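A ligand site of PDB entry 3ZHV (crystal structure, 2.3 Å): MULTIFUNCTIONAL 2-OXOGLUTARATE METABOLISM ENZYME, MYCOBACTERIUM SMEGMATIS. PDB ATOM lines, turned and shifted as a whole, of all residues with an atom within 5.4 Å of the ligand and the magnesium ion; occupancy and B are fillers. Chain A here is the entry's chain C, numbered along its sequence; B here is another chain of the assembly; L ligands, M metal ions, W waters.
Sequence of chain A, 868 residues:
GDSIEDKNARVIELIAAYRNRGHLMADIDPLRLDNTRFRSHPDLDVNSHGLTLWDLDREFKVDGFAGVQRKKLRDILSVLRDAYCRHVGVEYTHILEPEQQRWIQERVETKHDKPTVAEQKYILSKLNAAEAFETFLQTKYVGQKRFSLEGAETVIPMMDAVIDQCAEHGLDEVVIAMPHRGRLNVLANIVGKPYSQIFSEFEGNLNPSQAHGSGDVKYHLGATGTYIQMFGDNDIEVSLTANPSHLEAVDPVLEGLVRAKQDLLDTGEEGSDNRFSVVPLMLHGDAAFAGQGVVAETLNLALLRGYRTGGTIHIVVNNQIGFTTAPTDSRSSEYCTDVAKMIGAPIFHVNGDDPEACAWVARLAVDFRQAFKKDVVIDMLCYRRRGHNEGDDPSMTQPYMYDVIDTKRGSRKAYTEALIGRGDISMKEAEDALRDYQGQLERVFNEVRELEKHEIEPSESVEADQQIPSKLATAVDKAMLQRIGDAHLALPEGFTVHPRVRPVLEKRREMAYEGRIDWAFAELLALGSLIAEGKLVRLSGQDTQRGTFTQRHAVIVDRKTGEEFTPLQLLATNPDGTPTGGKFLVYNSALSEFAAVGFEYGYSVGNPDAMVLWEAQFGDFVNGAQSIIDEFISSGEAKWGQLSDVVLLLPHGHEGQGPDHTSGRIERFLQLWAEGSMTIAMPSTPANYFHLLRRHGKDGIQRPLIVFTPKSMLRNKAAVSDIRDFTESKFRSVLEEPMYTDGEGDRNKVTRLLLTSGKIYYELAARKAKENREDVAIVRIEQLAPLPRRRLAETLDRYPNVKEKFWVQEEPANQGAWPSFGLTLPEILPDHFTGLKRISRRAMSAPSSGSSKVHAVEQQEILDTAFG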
ATOM      1  N   HIS A 180     -11.495  23.812  29.626  1.00  0.00           N
ATOM      2  CA  HIS A 180     -12.444  24.882  29.240  1.00  0.00           C
ATOM      3  C   HIS A 180     -13.969  24.537  29.435  1.00  0.00           C
ATOM      4  O   HIS A 180     -14.745  25.475  29.630  1.00  0.00           O
ATOM      5  CB  HIS A 180     -12.212  25.326  27.776  1.00  0.00           C
ATOM      6  CG  HIS A 180     -12.382  24.214  26.781  1.00  0.00           C
ATOM      7  ND1 HIS A 180     -11.291  23.459  26.361  1.00  0.00           N
ATOM      8  CD2 HIS A 180     -13.511  23.704  26.216  1.00  0.00           C
ATOM      9  CE1 HIS A 180     -11.786  22.542  25.539  1.00  0.00           C
ATOM     10  NE2 HIS A 180     -13.118  22.645  25.437  1.00  0.00           N
ATOM     11  N   ARG A 181     -14.392  23.255  29.348  1.00  0.00           N
ATOM     12  CA  ARG A 181     -15.802  22.848  29.419  1.00  0.00           C
ATOM     13  C   ARG A 181     -16.500  23.237  30.759  1.00  0.00           C
ATOM     14  O   ARG A 181     -16.155  22.705  31.827  1.00  0.00           O
ATOM     15  CB  ARG A 181     -15.997  21.347  29.136  1.00  0.00           C
ATOM     16  CG  ARG A 181     -17.477  20.997  28.782  1.00  0.00           C
ATOM     17  CD  ARG A 181     -17.729  19.503  28.471  1.00  0.00           C
ATOM     18  NE  ARG A 181     -16.956  19.028  27.315  1.00  0.00           N
ATOM     19  CZ  ARG A 181     -17.275  19.295  26.044  1.00  0.00           C
ATOM     20  NH1 ARG A 181     -18.363  20.007  25.759  1.00  0.00           N
ATOM     21  NH2 ARG A 181     -16.522  18.833  25.057  1.00  0.00           N
ATOM     22  N   SER A 245      -4.635  25.488  26.407  1.00  0.00           N
ATOM     23  CA  SER A 245      -5.600  24.535  25.855  1.00  0.00           C
ATOM     24  C   SER A 245      -5.112  23.091  26.057  1.00  0.00           C
ATOM     25  O   SER A 245      -5.935  22.184  26.007  1.00  0.00           O
ATOM     26  CB  SER A 245      -5.839  24.793  24.373  1.00  0.00           C
ATOM     27  OG  SER A 245      -6.567  25.983  24.155  1.00  0.00           O
ATOM     28  N   HIS A 246      -3.781  22.913  26.312  1.00  0.00           N
ATOM     29  CA  HIS A 246      -3.118  21.625  26.564  1.00  0.00           C
ATOM     30  C   HIS A 246      -3.723  20.970  27.779  1.00  0.00           C
ATOM     31  O   HIS A 246      -3.459  21.387  28.916  1.00  0.00           O
ATOM     32  CB  HIS A 246      -1.605  21.822  26.744  1.00  0.00           C
ATOM     33  CG  HIS A 246      -0.912  22.214  25.476  1.00  0.00           C
ATOM     34  ND1 HIS A 246      -1.292  23.344  24.761  1.00  0.00           N
ATOM     35  CD2 HIS A 246       0.131  21.622  24.844  1.00  0.00           C
ATOM     36  CE1 HIS A 246      -0.488  23.388  23.708  1.00  0.00           C
ATOM     37  NE2 HIS A 246       0.399  22.394  23.721  1.00  0.00           N
ATOM     38  N   LEU A 247      -4.587  19.973  27.535  1.00  0.00           N
ATOM     39  CA  LEU A 247      -5.328  19.265  28.572  1.00  0.00           C
ATOM     40  C   LEU A 247      -4.374  18.561  29.516  1.00  0.00           C
ATOM     41  O   LEU A 247      -3.394  17.962  29.087  1.00  0.00           O
ATOM     42  CB  LEU A 247      -6.347  18.277  27.963  1.00  0.00           C
ATOM     43  CG  LEU A 247      -7.416  18.869  27.007  1.00  0.00           C
ATOM     44  CD1 LEU A 247      -8.138  17.767  26.219  1.00  0.00           C
ATOM     45  CD2 LEU A 247      -8.437  19.735  27.746  1.00  0.00           C
ATOM     46  N   GLY A 285     -11.351  15.682  31.920  1.00  0.00           N
ATOM     47  CA  GLY A 285     -12.138  15.029  30.880  1.00  0.00           C
ATOM     48  C   GLY A 285     -11.723  13.567  30.891  1.00  0.00           C
ATOM     49  O   GLY A 285     -10.589  13.245  31.275  1.00  0.00           O
ATOM     50  N   ASP A 286     -12.632  12.669  30.507  1.00  0.00           N
ATOM     51  CA  ASP A 286     -12.360  11.227  30.528  1.00  0.00           C
ATOM     52  C   ASP A 286     -11.252  10.798  29.548  1.00  0.00           C
ATOM     53  O   ASP A 286     -10.467   9.911  29.907  1.00  0.00           O
ATOM     54  CB  ASP A 286     -13.633  10.400  30.264  1.00  0.00           C
ATOM     55  CG  ASP A 286     -14.373  10.736  28.985  1.00  0.00           C
ATOM     56  OD1 ASP A 286     -14.760  11.922  28.803  1.00  0.00           O
ATOM     57  OD2 ASP A 286     -14.611   9.807  28.178  1.00  0.00           O
ATOM     58  N   ALA A 287     -11.189  11.391  28.321  1.00  0.00           N
ATOM     59  CA  ALA A 287     -10.166  10.934  27.370  1.00  0.00           C
ATOM     60  C   ALA A 287      -8.789  11.406  27.807  1.00  0.00           C
ATOM     61  O   ALA A 287      -7.860  10.618  27.801  1.00  0.00           O
ATOM     62  CB  ALA A 287     -10.480  11.400  25.943  1.00  0.00           C
ATOM     63  N   ALA A 288      -8.689  12.671  28.275  1.00  0.00           N
ATOM     64  CA  ALA A 288      -7.443  13.305  28.711  1.00  0.00           C
ATOM     65  C   ALA A 288      -6.885  12.668  29.993  1.00  0.00           C
ATOM     66  O   ALA A 288      -5.682  12.476  30.080  1.00  0.00           O
ATOM     67  CB  ALA A 288      -7.670  14.803  28.927  1.00  0.00           C
ATOM     68  N   PHE A 289      -7.750  12.330  30.954  1.00  0.00           N
ATOM     69  CA  PHE A 289      -7.347  11.737  32.224  1.00  0.00           C
ATOM     70  C   PHE A 289      -6.667  10.389  32.016  1.00  0.00           C
ATOM     71  O   PHE A 289      -5.724  10.086  32.746  1.00  0.00           O
ATOM     72  CB  PHE A 289      -8.559  11.572  33.174  1.00  0.00           C
ATOM     73  CG  PHE A 289      -8.141  11.368  34.619  1.00  0.00           C
ATOM     74  CD1 PHE A 289      -7.551  12.384  35.341  1.00  0.00           C
ATOM     75  CD2 PHE A 289      -8.323  10.141  35.240  1.00  0.00           C
ATOM     76  CE1 PHE A 289      -7.172  12.203  36.668  1.00  0.00           C
ATOM     77  CE2 PHE A 289      -7.939   9.948  36.578  1.00  0.00           C
ATOM     78  CZ  PHE A 289      -7.361  10.979  37.278  1.00  0.00           C
ATOM     79  N   GLN A 292      -3.118  11.276  29.043  1.00  0.00           N
ATOM     80  CA  GLN A 292      -2.021  12.215  29.301  1.00  0.00           C
ATOM     81  C   GLN A 292      -1.129  11.713  30.433  1.00  0.00           C
ATOM     82  O   GLN A 292      -1.624  11.495  31.542  1.00  0.00           O
ATOM     83  CB  GLN A 292      -2.569  13.628  29.606  1.00  0.00           C
ATOM     84  CG  GLN A 292      -3.147  14.332  28.380  1.00  0.00           C
ATOM     85  CD  GLN A 292      -2.094  14.659  27.334  1.00  0.00           C
ATOM     86  OE1 GLN A 292      -1.104  15.338  27.593  1.00  0.00           O
ATOM     87  NE2 GLN A 292      -2.267  14.155  26.122  1.00  0.00           N
ATOM     88  N   VAL A 317     -15.202  14.639  34.482  1.00  0.00           N
ATOM     89  CA  VAL A 317     -16.451  14.873  33.762  1.00  0.00           C
ATOM     90  C   VAL A 317     -16.426  13.832  32.650  1.00  0.00           C
ATOM     91  O   VAL A 317     -15.892  14.080  31.545  1.00  0.00           O
ATOM     92  CB  VAL A 317     -16.607  16.341  33.272  1.00  0.00           C
ATOM     93  CG1 VAL A 317     -17.927  16.534  32.533  1.00  0.00           C
ATOM     94  CG2 VAL A 317     -16.514  17.316  34.452  1.00  0.00           C
ATOM     95  N   ASN A 319     -18.031  12.166  30.131  1.00  0.00           N
ATOM     96  CA  ASN A 319     -19.128  12.236  29.193  1.00  0.00           C
ATOM     97  C   ASN A 319     -19.026  11.129  28.143  1.00  0.00           C
ATOM     98  O   ASN A 319     -19.736  11.161  27.148  1.00  0.00           O
ATOM     99  CB  ASN A 319     -19.246  13.621  28.558  1.00  0.00           C
ATOM    100  CG  ASN A 319     -17.992  14.135  27.888  1.00  0.00           C
ATOM    101  OD1 ASN A 319     -17.070  13.375  27.537  1.00  0.00           O
ATOM    102  ND2 ASN A 319     -17.952  15.448  27.690  1.00  0.00           N
ATOM    103  N   GLN A 320     -18.145  10.133  28.418  1.00  0.00           N
ATOM    104  CA  GLN A 320     -17.944   8.869  27.678  1.00  0.00           C
ATOM    105  C   GLN A 320     -17.650   9.119  26.198  1.00  0.00           C
ATOM    106  O   GLN A 320     -18.056   8.343  25.334  1.00  0.00           O
ATOM    107  CB  GLN A 320     -19.182   7.942  27.845  1.00  0.00           C
ATOM    108  CG  GLN A 320     -19.718   7.856  29.299  1.00  0.00           C
ATOM    109  CD  GLN A 320     -20.998   7.057  29.427  1.00  0.00           C
ATOM    110  OE1 GLN A 320     -21.021   5.850  29.201  1.00  0.00           O
ATOM    111  NE2 GLN A 320     -22.068   7.702  29.842  1.00  0.00           N
ATOM    112  N   ILE A 321     -16.956  10.214  25.912  1.00  0.00           N
ATOM    113  CA  ILE A 321     -16.555  10.608  24.564  1.00  0.00           C
ATOM    114  C   ILE A 321     -15.383  11.590  24.679  1.00  0.00           C
ATOM    115  O   ILE A 321     -15.215  12.276  25.705  1.00  0.00           O
ATOM    116  CB  ILE A 321     -17.753  11.173  23.722  1.00  0.00           C
ATOM    117  CG1 ILE A 321     -17.428  11.185  22.201  1.00  0.00           C
ATOM    118  CG2 ILE A 321     -18.324  12.515  24.268  1.00  0.00           C
ATOM    119  CD1 ILE A 321     -18.636  11.307  21.267  1.00  0.00           C
ATOM    120  N   GLY A 322     -14.553  11.586  23.641  1.00  0.00           N
ATOM    121  CA  GLY A 322     -13.419  12.490  23.490  1.00  0.00           C
ATOM    122  C   GLY A 322     -13.391  12.971  22.059  1.00  0.00           C
ATOM    123  O   GLY A 322     -12.828  12.281  21.203  1.00  0.00           O
ATOM    124  N   PHE A 323     -14.097  14.104  21.795  1.00  0.00           N
ATOM    125  CA  PHE A 323     -14.310  14.706  20.459  1.00  0.00           C
ATOM    126  C   PHE A 323     -15.159  13.714  19.611  1.00  0.00           C
ATOM    127  O   PHE A 323     -16.373  13.666  19.771  1.00  0.00           O
ATOM    128  CB  PHE A 323     -12.942  15.123  19.817  1.00  0.00           C
ATOM    129  CG  PHE A 323     -12.983  16.140  18.707  1.00  0.00           C
ATOM    130  CD1 PHE A 323     -14.039  16.177  17.786  1.00  0.00           C
ATOM    131  CD2 PHE A 323     -11.941  17.040  18.534  1.00  0.00           C
ATOM    132  CE1 PHE A 323     -14.069  17.127  16.760  1.00  0.00           C
ATOM    133  CE2 PHE A 323     -11.978  18.003  17.506  1.00  0.00           C
ATOM    134  CZ  PHE A 323     -13.033  18.028  16.626  1.00  0.00           C
ATOM    135  N   ARG A 384     -22.457  14.366  26.652  1.00  0.00           N
ATOM    136  CA  ARG A 384     -22.249  15.627  25.984  1.00  0.00           C
ATOM    137  C   ARG A 384     -23.441  15.797  25.031  1.00  0.00           C
ATOM    138  O   ARG A 384     -23.445  15.179  23.955  1.00  0.00           O
ATOM    139  CB  ARG A 384     -20.881  15.567  25.262  1.00  0.00           C
ATOM    140  CG  ARG A 384     -20.312  16.908  24.802  1.00  0.00           C
ATOM    141  CD  ARG A 384     -19.243  16.679  23.771  1.00  0.00           C
ATOM    142  NE  ARG A 384     -19.841  16.183  22.531  1.00  0.00           N
ATOM    143  CZ  ARG A 384     -19.183  15.550  21.566  1.00  0.00           C
ATOM    144  NH1 ARG A 384     -17.892  15.281  21.696  1.00  0.00           N
ATOM    145  NH2 ARG A 384     -19.814  15.155  20.470  1.00  0.00           N
ATOM    146  N   HIS A 388     -19.043  18.266  19.541  1.00  0.00           N
ATOM    147  CA  HIS A 388     -17.798  18.827  20.059  1.00  0.00           C
ATOM    148  C   HIS A 388     -17.644  20.317  19.721  1.00  0.00           C
ATOM    149  O   HIS A 388     -17.170  21.063  20.565  1.00  0.00           O
ATOM    150  CB  HIS A 388     -16.553  18.060  19.570  1.00  0.00           C
ATOM    151  CG  HIS A 388     -15.339  18.375  20.393  1.00  0.00           C
ATOM    152  ND1 HIS A 388     -15.157  17.814  21.663  1.00  0.00           N
ATOM    153  CD2 HIS A 388     -14.330  19.233  20.146  1.00  0.00           C
ATOM    154  CE1 HIS A 388     -14.023  18.324  22.117  1.00  0.00           C
ATOM    155  NE2 HIS A 388     -13.492  19.184  21.240  1.00  0.00           N
ATOM    156  N   GLN B 542      -5.378  11.923  16.719  1.00  0.00           N
ATOM    157  CA  GLN B 542      -6.635  12.232  17.390  1.00  0.00           C
ATOM    158  C   GLN B 542      -7.748  12.536  16.384  1.00  0.00           C
ATOM    159  O   GLN B 542      -7.617  13.458  15.562  1.00  0.00           O
ATOM    160  CB  GLN B 542      -6.437  13.368  18.388  1.00  0.00           C
ATOM    161  CG  GLN B 542      -5.802  12.905  19.697  1.00  0.00           C
ATOM    162  CD  GLN B 542      -4.928  13.977  20.315  1.00  0.00           C
ATOM    163  OE1 GLN B 542      -5.183  15.176  20.191  1.00  0.00           O
ATOM    164  NE2 GLN B 542      -3.872  13.569  21.002  1.00  0.00           N
ATOM    165  N   ASP B 543      -8.804  11.685  16.382  1.00  0.00           N
ATOM    166  CA  ASP B 543      -9.997  11.781  15.512  1.00  0.00           C
ATOM    167  C   ASP B 543      -9.637  11.783  14.016  1.00  0.00           C
ATOM    168  O   ASP B 543     -10.368  12.338  13.197  1.00  0.00           O
ATOM    169  CB  ASP B 543     -10.844  13.028  15.882  1.00  0.00           C
ATOM    170  CG  ASP B 543     -11.098  13.142  17.379  1.00  0.00           C
ATOM    171  OD1 ASP B 543     -11.955  12.360  17.897  1.00  0.00           O
ATOM    172  OD2 ASP B 543     -10.348  13.894  18.068  1.00  0.00           O
ATOM    173  N   LEU B 591      -5.720   9.960  23.685  1.00  0.00           N
ATOM    174  CA  LEU B 591      -5.389  11.361  23.838  1.00  0.00           C
ATOM    175  C   LEU B 591      -3.949  11.490  24.393  1.00  0.00           C
ATOM    176  O   LEU B 591      -3.734  11.890  25.543  1.00  0.00           O
ATOM    177  CB  LEU B 591      -6.428  12.063  24.740  1.00  0.00           C
ATOM    178  CG  LEU B 591      -6.708  13.522  24.435  1.00  0.00           C
ATOM    179  CD1 LEU B 591      -8.037  13.917  24.982  1.00  0.00           C
ATOM    180  CD2 LEU B 591      -5.562  14.464  24.951  1.00  0.00           C
ATOM    181  N   GLU B 593       0.330  12.342  22.944  1.00  0.00           N
ATOM    182  CA  GLU B 593       1.204  12.855  21.909  1.00  0.00           C
ATOM    183  C   GLU B 593       2.510  12.114  22.003  1.00  0.00           C
ATOM    184  O   GLU B 593       2.900  11.496  21.031  1.00  0.00           O
ATOM    185  CB  GLU B 593       1.402  14.389  22.010  1.00  0.00           C
ATOM    186  CG  GLU B 593       0.198  15.169  21.505  1.00  0.00           C
ATOM    187  CD  GLU B 593      -0.940  15.316  22.488  1.00  0.00           C
ATOM    188  OE1 GLU B 593      -0.689  15.298  23.714  1.00  0.00           O
ATOM    189  OE2 GLU B 593      -2.098  15.447  22.035  1.00  0.00           O
ATOM    190  N   GLN B 617      -3.769  16.918  16.393  1.00  0.00           N
ATOM    191  CA  GLN B 617      -5.107  17.501  16.350  1.00  0.00           C
ATOM    192  C   GLN B 617      -4.981  18.910  15.747  1.00  0.00           C
ATOM    193  O   GLN B 617      -5.708  19.278  14.812  1.00  0.00           O
ATOM    194  CB  GLN B 617      -5.758  17.501  17.745  1.00  0.00           C
ATOM    195  CG  GLN B 617      -7.188  18.058  17.710  1.00  0.00           C
ATOM    196  CD  GLN B 617      -8.223  17.030  18.008  1.00  0.00           C
ATOM    197  OE1 GLN B 617      -8.700  16.911  19.127  1.00  0.00           O
ATOM    198  NE2 GLN B 617      -8.628  16.266  17.013  1.00  0.00           N
ATOM    199  N   PHE B 618      -4.001  19.650  16.276  1.00  0.00           N
ATOM    200  CA  PHE B 618      -3.483  20.964  15.901  1.00  0.00           C
ATOM    201  C   PHE B 618      -2.004  20.837  16.104  1.00  0.00           C
ATOM    202  O   PHE B 618      -1.611  20.158  17.052  1.00  0.00           O
ATOM    203  CB  PHE B 618      -4.093  22.083  16.781  1.00  0.00           C
ATOM    204  CG  PHE B 618      -5.514  22.445  16.428  1.00  0.00           C
ATOM    205  CD1 PHE B 618      -6.586  21.726  16.956  1.00  0.00           C
ATOM    206  CD2 PHE B 618      -5.786  23.535  15.608  1.00  0.00           C
ATOM    207  CE1 PHE B 618      -7.902  22.067  16.638  1.00  0.00           C
ATOM    208  CE2 PHE B 618      -7.110  23.889  15.299  1.00  0.00           C
ATOM    209  CZ  PHE B 618      -8.154  23.151  15.811  1.00  0.00           C
ATOM    210  N   PHE B 621      -0.018  21.002  19.761  1.00  0.00           N
ATOM    211  CA  PHE B 621       0.043  19.980  20.793  1.00  0.00           C
ATOM    212  C   PHE B 621       1.172  18.993  20.597  1.00  0.00           C
ATOM    213  O   PHE B 621       1.406  18.163  21.476  1.00  0.00           O
ATOM    214  CB  PHE B 621      -1.310  19.234  20.880  1.00  0.00           C
ATOM    215  CG  PHE B 621      -2.450  20.182  21.147  1.00  0.00           C
ATOM    216  CD1 PHE B 621      -2.512  20.911  22.333  1.00  0.00           C
ATOM    217  CD2 PHE B 621      -3.449  20.369  20.210  1.00  0.00           C
ATOM    218  CE1 PHE B 621      -3.546  21.808  22.565  1.00  0.00           C
ATOM    219  CE2 PHE B 621      -4.479  21.276  20.432  1.00  0.00           C
ATOM    220  CZ  PHE B 621      -4.538  21.983  21.618  1.00  0.00           C
ATOM    221  N   HIS B 661      -4.034  26.965  19.064  1.00  0.00           N
ATOM    222  CA  HIS B 661      -4.751  26.512  17.867  1.00  0.00           C
ATOM    223  C   HIS B 661      -4.274  27.351  16.670  1.00  0.00           C
ATOM    224  O   HIS B 661      -5.087  27.712  15.804  1.00  0.00           O
ATOM    225  CB  HIS B 661      -6.278  26.626  18.051  1.00  0.00           C
ATOM    226  CG  HIS B 661      -6.788  25.778  19.163  1.00  0.00           C
ATOM    227  ND1 HIS B 661      -6.931  26.279  20.454  1.00  0.00           N
ATOM    228  CD2 HIS B 661      -7.123  24.470  19.149  1.00  0.00           C
ATOM    229  CE1 HIS B 661      -7.370  25.270  21.186  1.00  0.00           C
ATOM    230  NE2 HIS B 661      -7.495  24.151  20.449  1.00  0.00           N
HETATM  231  S1  LIG L   1     -10.586  18.645  22.908  1.00  0.00           S
HETATM  232  C1  LIG L   1      -9.278  19.299  22.212  1.00  0.00           C
HETATM  233  N1  LIG L   1      -8.247  18.309  21.961  1.00  0.00           N
HETATM  234  C2  LIG L   1      -8.725  17.037  22.290  1.00  0.00           C
HETATM  235  C3  LIG L   1     -10.011  17.076  22.842  1.00  0.00           C
HETATM  236  C4  LIG L   1     -10.793  15.837  23.301  1.00  0.00           C
HETATM  237  C5  LIG L   1     -11.112  15.970  24.779  1.00  0.00           C
HETATM  238  O1  LIG L   1     -11.532  14.708  25.378  1.00  0.00           O
HETATM  239  P1  LIG L   1     -11.981  14.647  26.934  1.00  0.00           P
HETATM  240  P2  LIG L   1     -14.408  16.535  26.711  1.00  0.00           P
HETATM  241  N2  LIG L   1      -3.872  17.156  23.278  1.00  0.00           N
HETATM  242  O2  LIG L   1     -10.873  14.647  27.932  1.00  0.00           O
HETATM  243  O3  LIG L   1     -14.681  17.312  27.998  1.00  0.00           O
HETATM  244  C6  LIG L   1      -3.816  17.978  24.336  1.00  0.00           C
HETATM  245  C7  LIG L   1      -9.259  20.729  21.595  1.00  0.00           C
HETATM  246  O4  LIG L   1      -8.220  21.632  21.966  1.00  0.00           O
HETATM  247  C8  LIG L   1      -9.418  20.672  20.090  1.00  0.00           C
HETATM  248  O5  LIG L   1     -12.921  13.440  26.946  1.00  0.00           O
HETATM  249  O6  LIG L   1     -14.023  17.472  25.549  1.00  0.00           O
HETATM  250  N3  LIG L   1      -4.633  19.011  24.574  1.00  0.00           N
HETATM  251  O7  LIG L   1     -13.068  15.771  26.961  1.00  0.00           O
HETATM  252  O8  LIG L   1     -15.446  15.516  26.393  1.00  0.00           O
HETATM  253  C9  LIG L   1      -5.628  19.237  23.687  1.00  0.00           C
HETATM  254  N4  LIG L   1      -6.477  20.226  23.982  1.00  0.00           N
HETATM  255  C10 LIG L   1      -5.786  18.415  22.534  1.00  0.00           C
HETATM  256  C11 LIG L   1      -4.863  17.402  22.401  1.00  0.00           C
HETATM  257  C12 LIG L   1      -6.865  18.564  21.486  1.00  0.00           C
HETATM  258  C13 LIG L   1      -2.773  17.694  25.362  1.00  0.00           C
HETATM  259  C14 LIG L   1      -7.986  15.779  21.916  1.00  0.00           C
HETATM  260 MG    MG M   1     -14.944  13.444  27.288  1.00  0.00          MG
HETATM  261  O   HOH W   1     -15.089  14.530  29.110  1.00  0.00           O
HETATM  262  O   HOH W   2     -10.454  17.277  29.086  1.00  0.00           O
HETATM  263  O   HOH W   3     -12.537  19.416  26.300  1.00  0.00           O
HETATM  264  O   HOH W   4     -13.193  18.526  29.533  1.00  0.00           O
HETATM  265  O   HOH W   5     -15.825  15.618  23.432  1.00  0.00           O
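Of the 27 residues printed, 3 come within 4 Å of the magnesium ion.
A nitrogen (N2) of the ligand lies within hydrogen-bond range of the side-chain carboxylate (OE2) of Glu 593 of chain B, 2.8 Å away. The backbone carbonyl oxygen (O) of Ser 245 lies within hydrogen-bond range of a nitrogen (N4) of the ligand (2.9 Å). NH2 of Arg 181 lies within salt-bridge range of O6 of the ligand (2.9 Å). The backbone NH (N) of Ala 288 is in hydrogen-bond range of an oxygen (O2) of the ligand, 3.0 Å away. N of Ala 287 is in hydrogen-bond range of O2 of the ligand (3.3 Å). An oxygen (O4) of the ligand lies within hydrogen-bond range of a ring nitrogen (NE2) of His 661 of chain B, 3.0 Å away. N of Leu 247 is in hydrogen-bond range of N3 of the ligand (3.1 Å). A ring nitrogen (NE2) of His 388 sits close to a sulfur (S1) of the ligand.
Water W1 lies within hydrogen-bond range of O of Val 317 (2.6 Å), O3 of the ligand (3.0 Å), ND2 of Asn 319 (3.3 Å) and N of Asp 286 (3.4 Å). Water W3 bridges an oxygen (O6) of the ligand (2.6 Å) and a ring nitrogen (NE2) of His 180 (3.4 Å). Water W2 bridges an oxygen (O2) of the ligand and the backbone NH of Gly 285. Water W5 lies within hydrogen-bond range of the guanidinium group of Arg 384 (2.7 Å), the backbone NH of Phe 323 (2.8 Å), a ring nitrogen (ND1) of His 388 (2.9 Å) and an oxygen (O6) of the ligand (3.3 Å).
The side-chain carboxylate (OE2) of Glu 593 of chain B lies within hydrogen-bond range of the side-chain amide nitrogen (NE2) of Gln 542 of chain B. The side-chain amide nitrogen (NE2) of Gln 292 is in hydrogen-bond range of the side-chain carboxylate (OE1) of Glu 593 of chain B (3.1 Å). NE2 of Gln 617 of chain B sits at hydrogen-bond distance from O of Gln 542 of chain B, at 3.3 Å. The side-chain carboxylate (OD2) of Asp 543 of chain B sits at hydrogen-bond distance from the side-chain amide nitrogen (NE2) of Gln 617 of chain B (3.1 Å). The backbone carbonyl oxygen of Leu 591 of chain B sits at hydrogen-bond distance from the side-chain amide nitrogen of Gln 292 (2.8 Å).
OE1 of Gln 617 of chain B sits close to N1 of the ligand (3.2 Å). CA of His 246 touches N3 of the ligand, 3.6 Å away. CA of Gly 285 touches O2 of the ligand, at 3.2 Å. Gln 292 touches the ligand. CA of Gly 322 touches O1 of the ligand (3.5 Å). Gln 542 of chain B touches the ligand (OE1 to C11, 3.2 Å). CD1 of Leu 591 of chain B touches C14 of the ligand, at 3.6 Å. CE1 of Phe 621 of chain B touches C9 of the ligand, 3.5 Å away. Hydrophobic or aromatic side chains that line the ligand: Leu 247, Ala 287, Ala 288, His 388, Leu 591 of chain B, Phe 621 of chain B and His 661 of chain B. Along chain A the residues within 4 Å of the ligand span positions 181 to 388. The nearest printed residue that does not touch the ligand is Phe 618 of chain B (4.02 Å).
O of Ile 321 binds the magnesium ion, 2.0 Å away. The magnesium ion is bound by O5 of the ligand, at 2.1 Å. The magnesium ion is bound by water W1, 2.1 Å away. The magnesium ion is bound by the side-chain amide oxygen (OD1) of Asn 319, 2.1 Å away. The side-chain carboxylate (OD1) of Asp 286 is bound to the magnesium ion, 2.2 Å away. O8 of the ligand is bound to the magnesium ion, 2.3 Å away.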
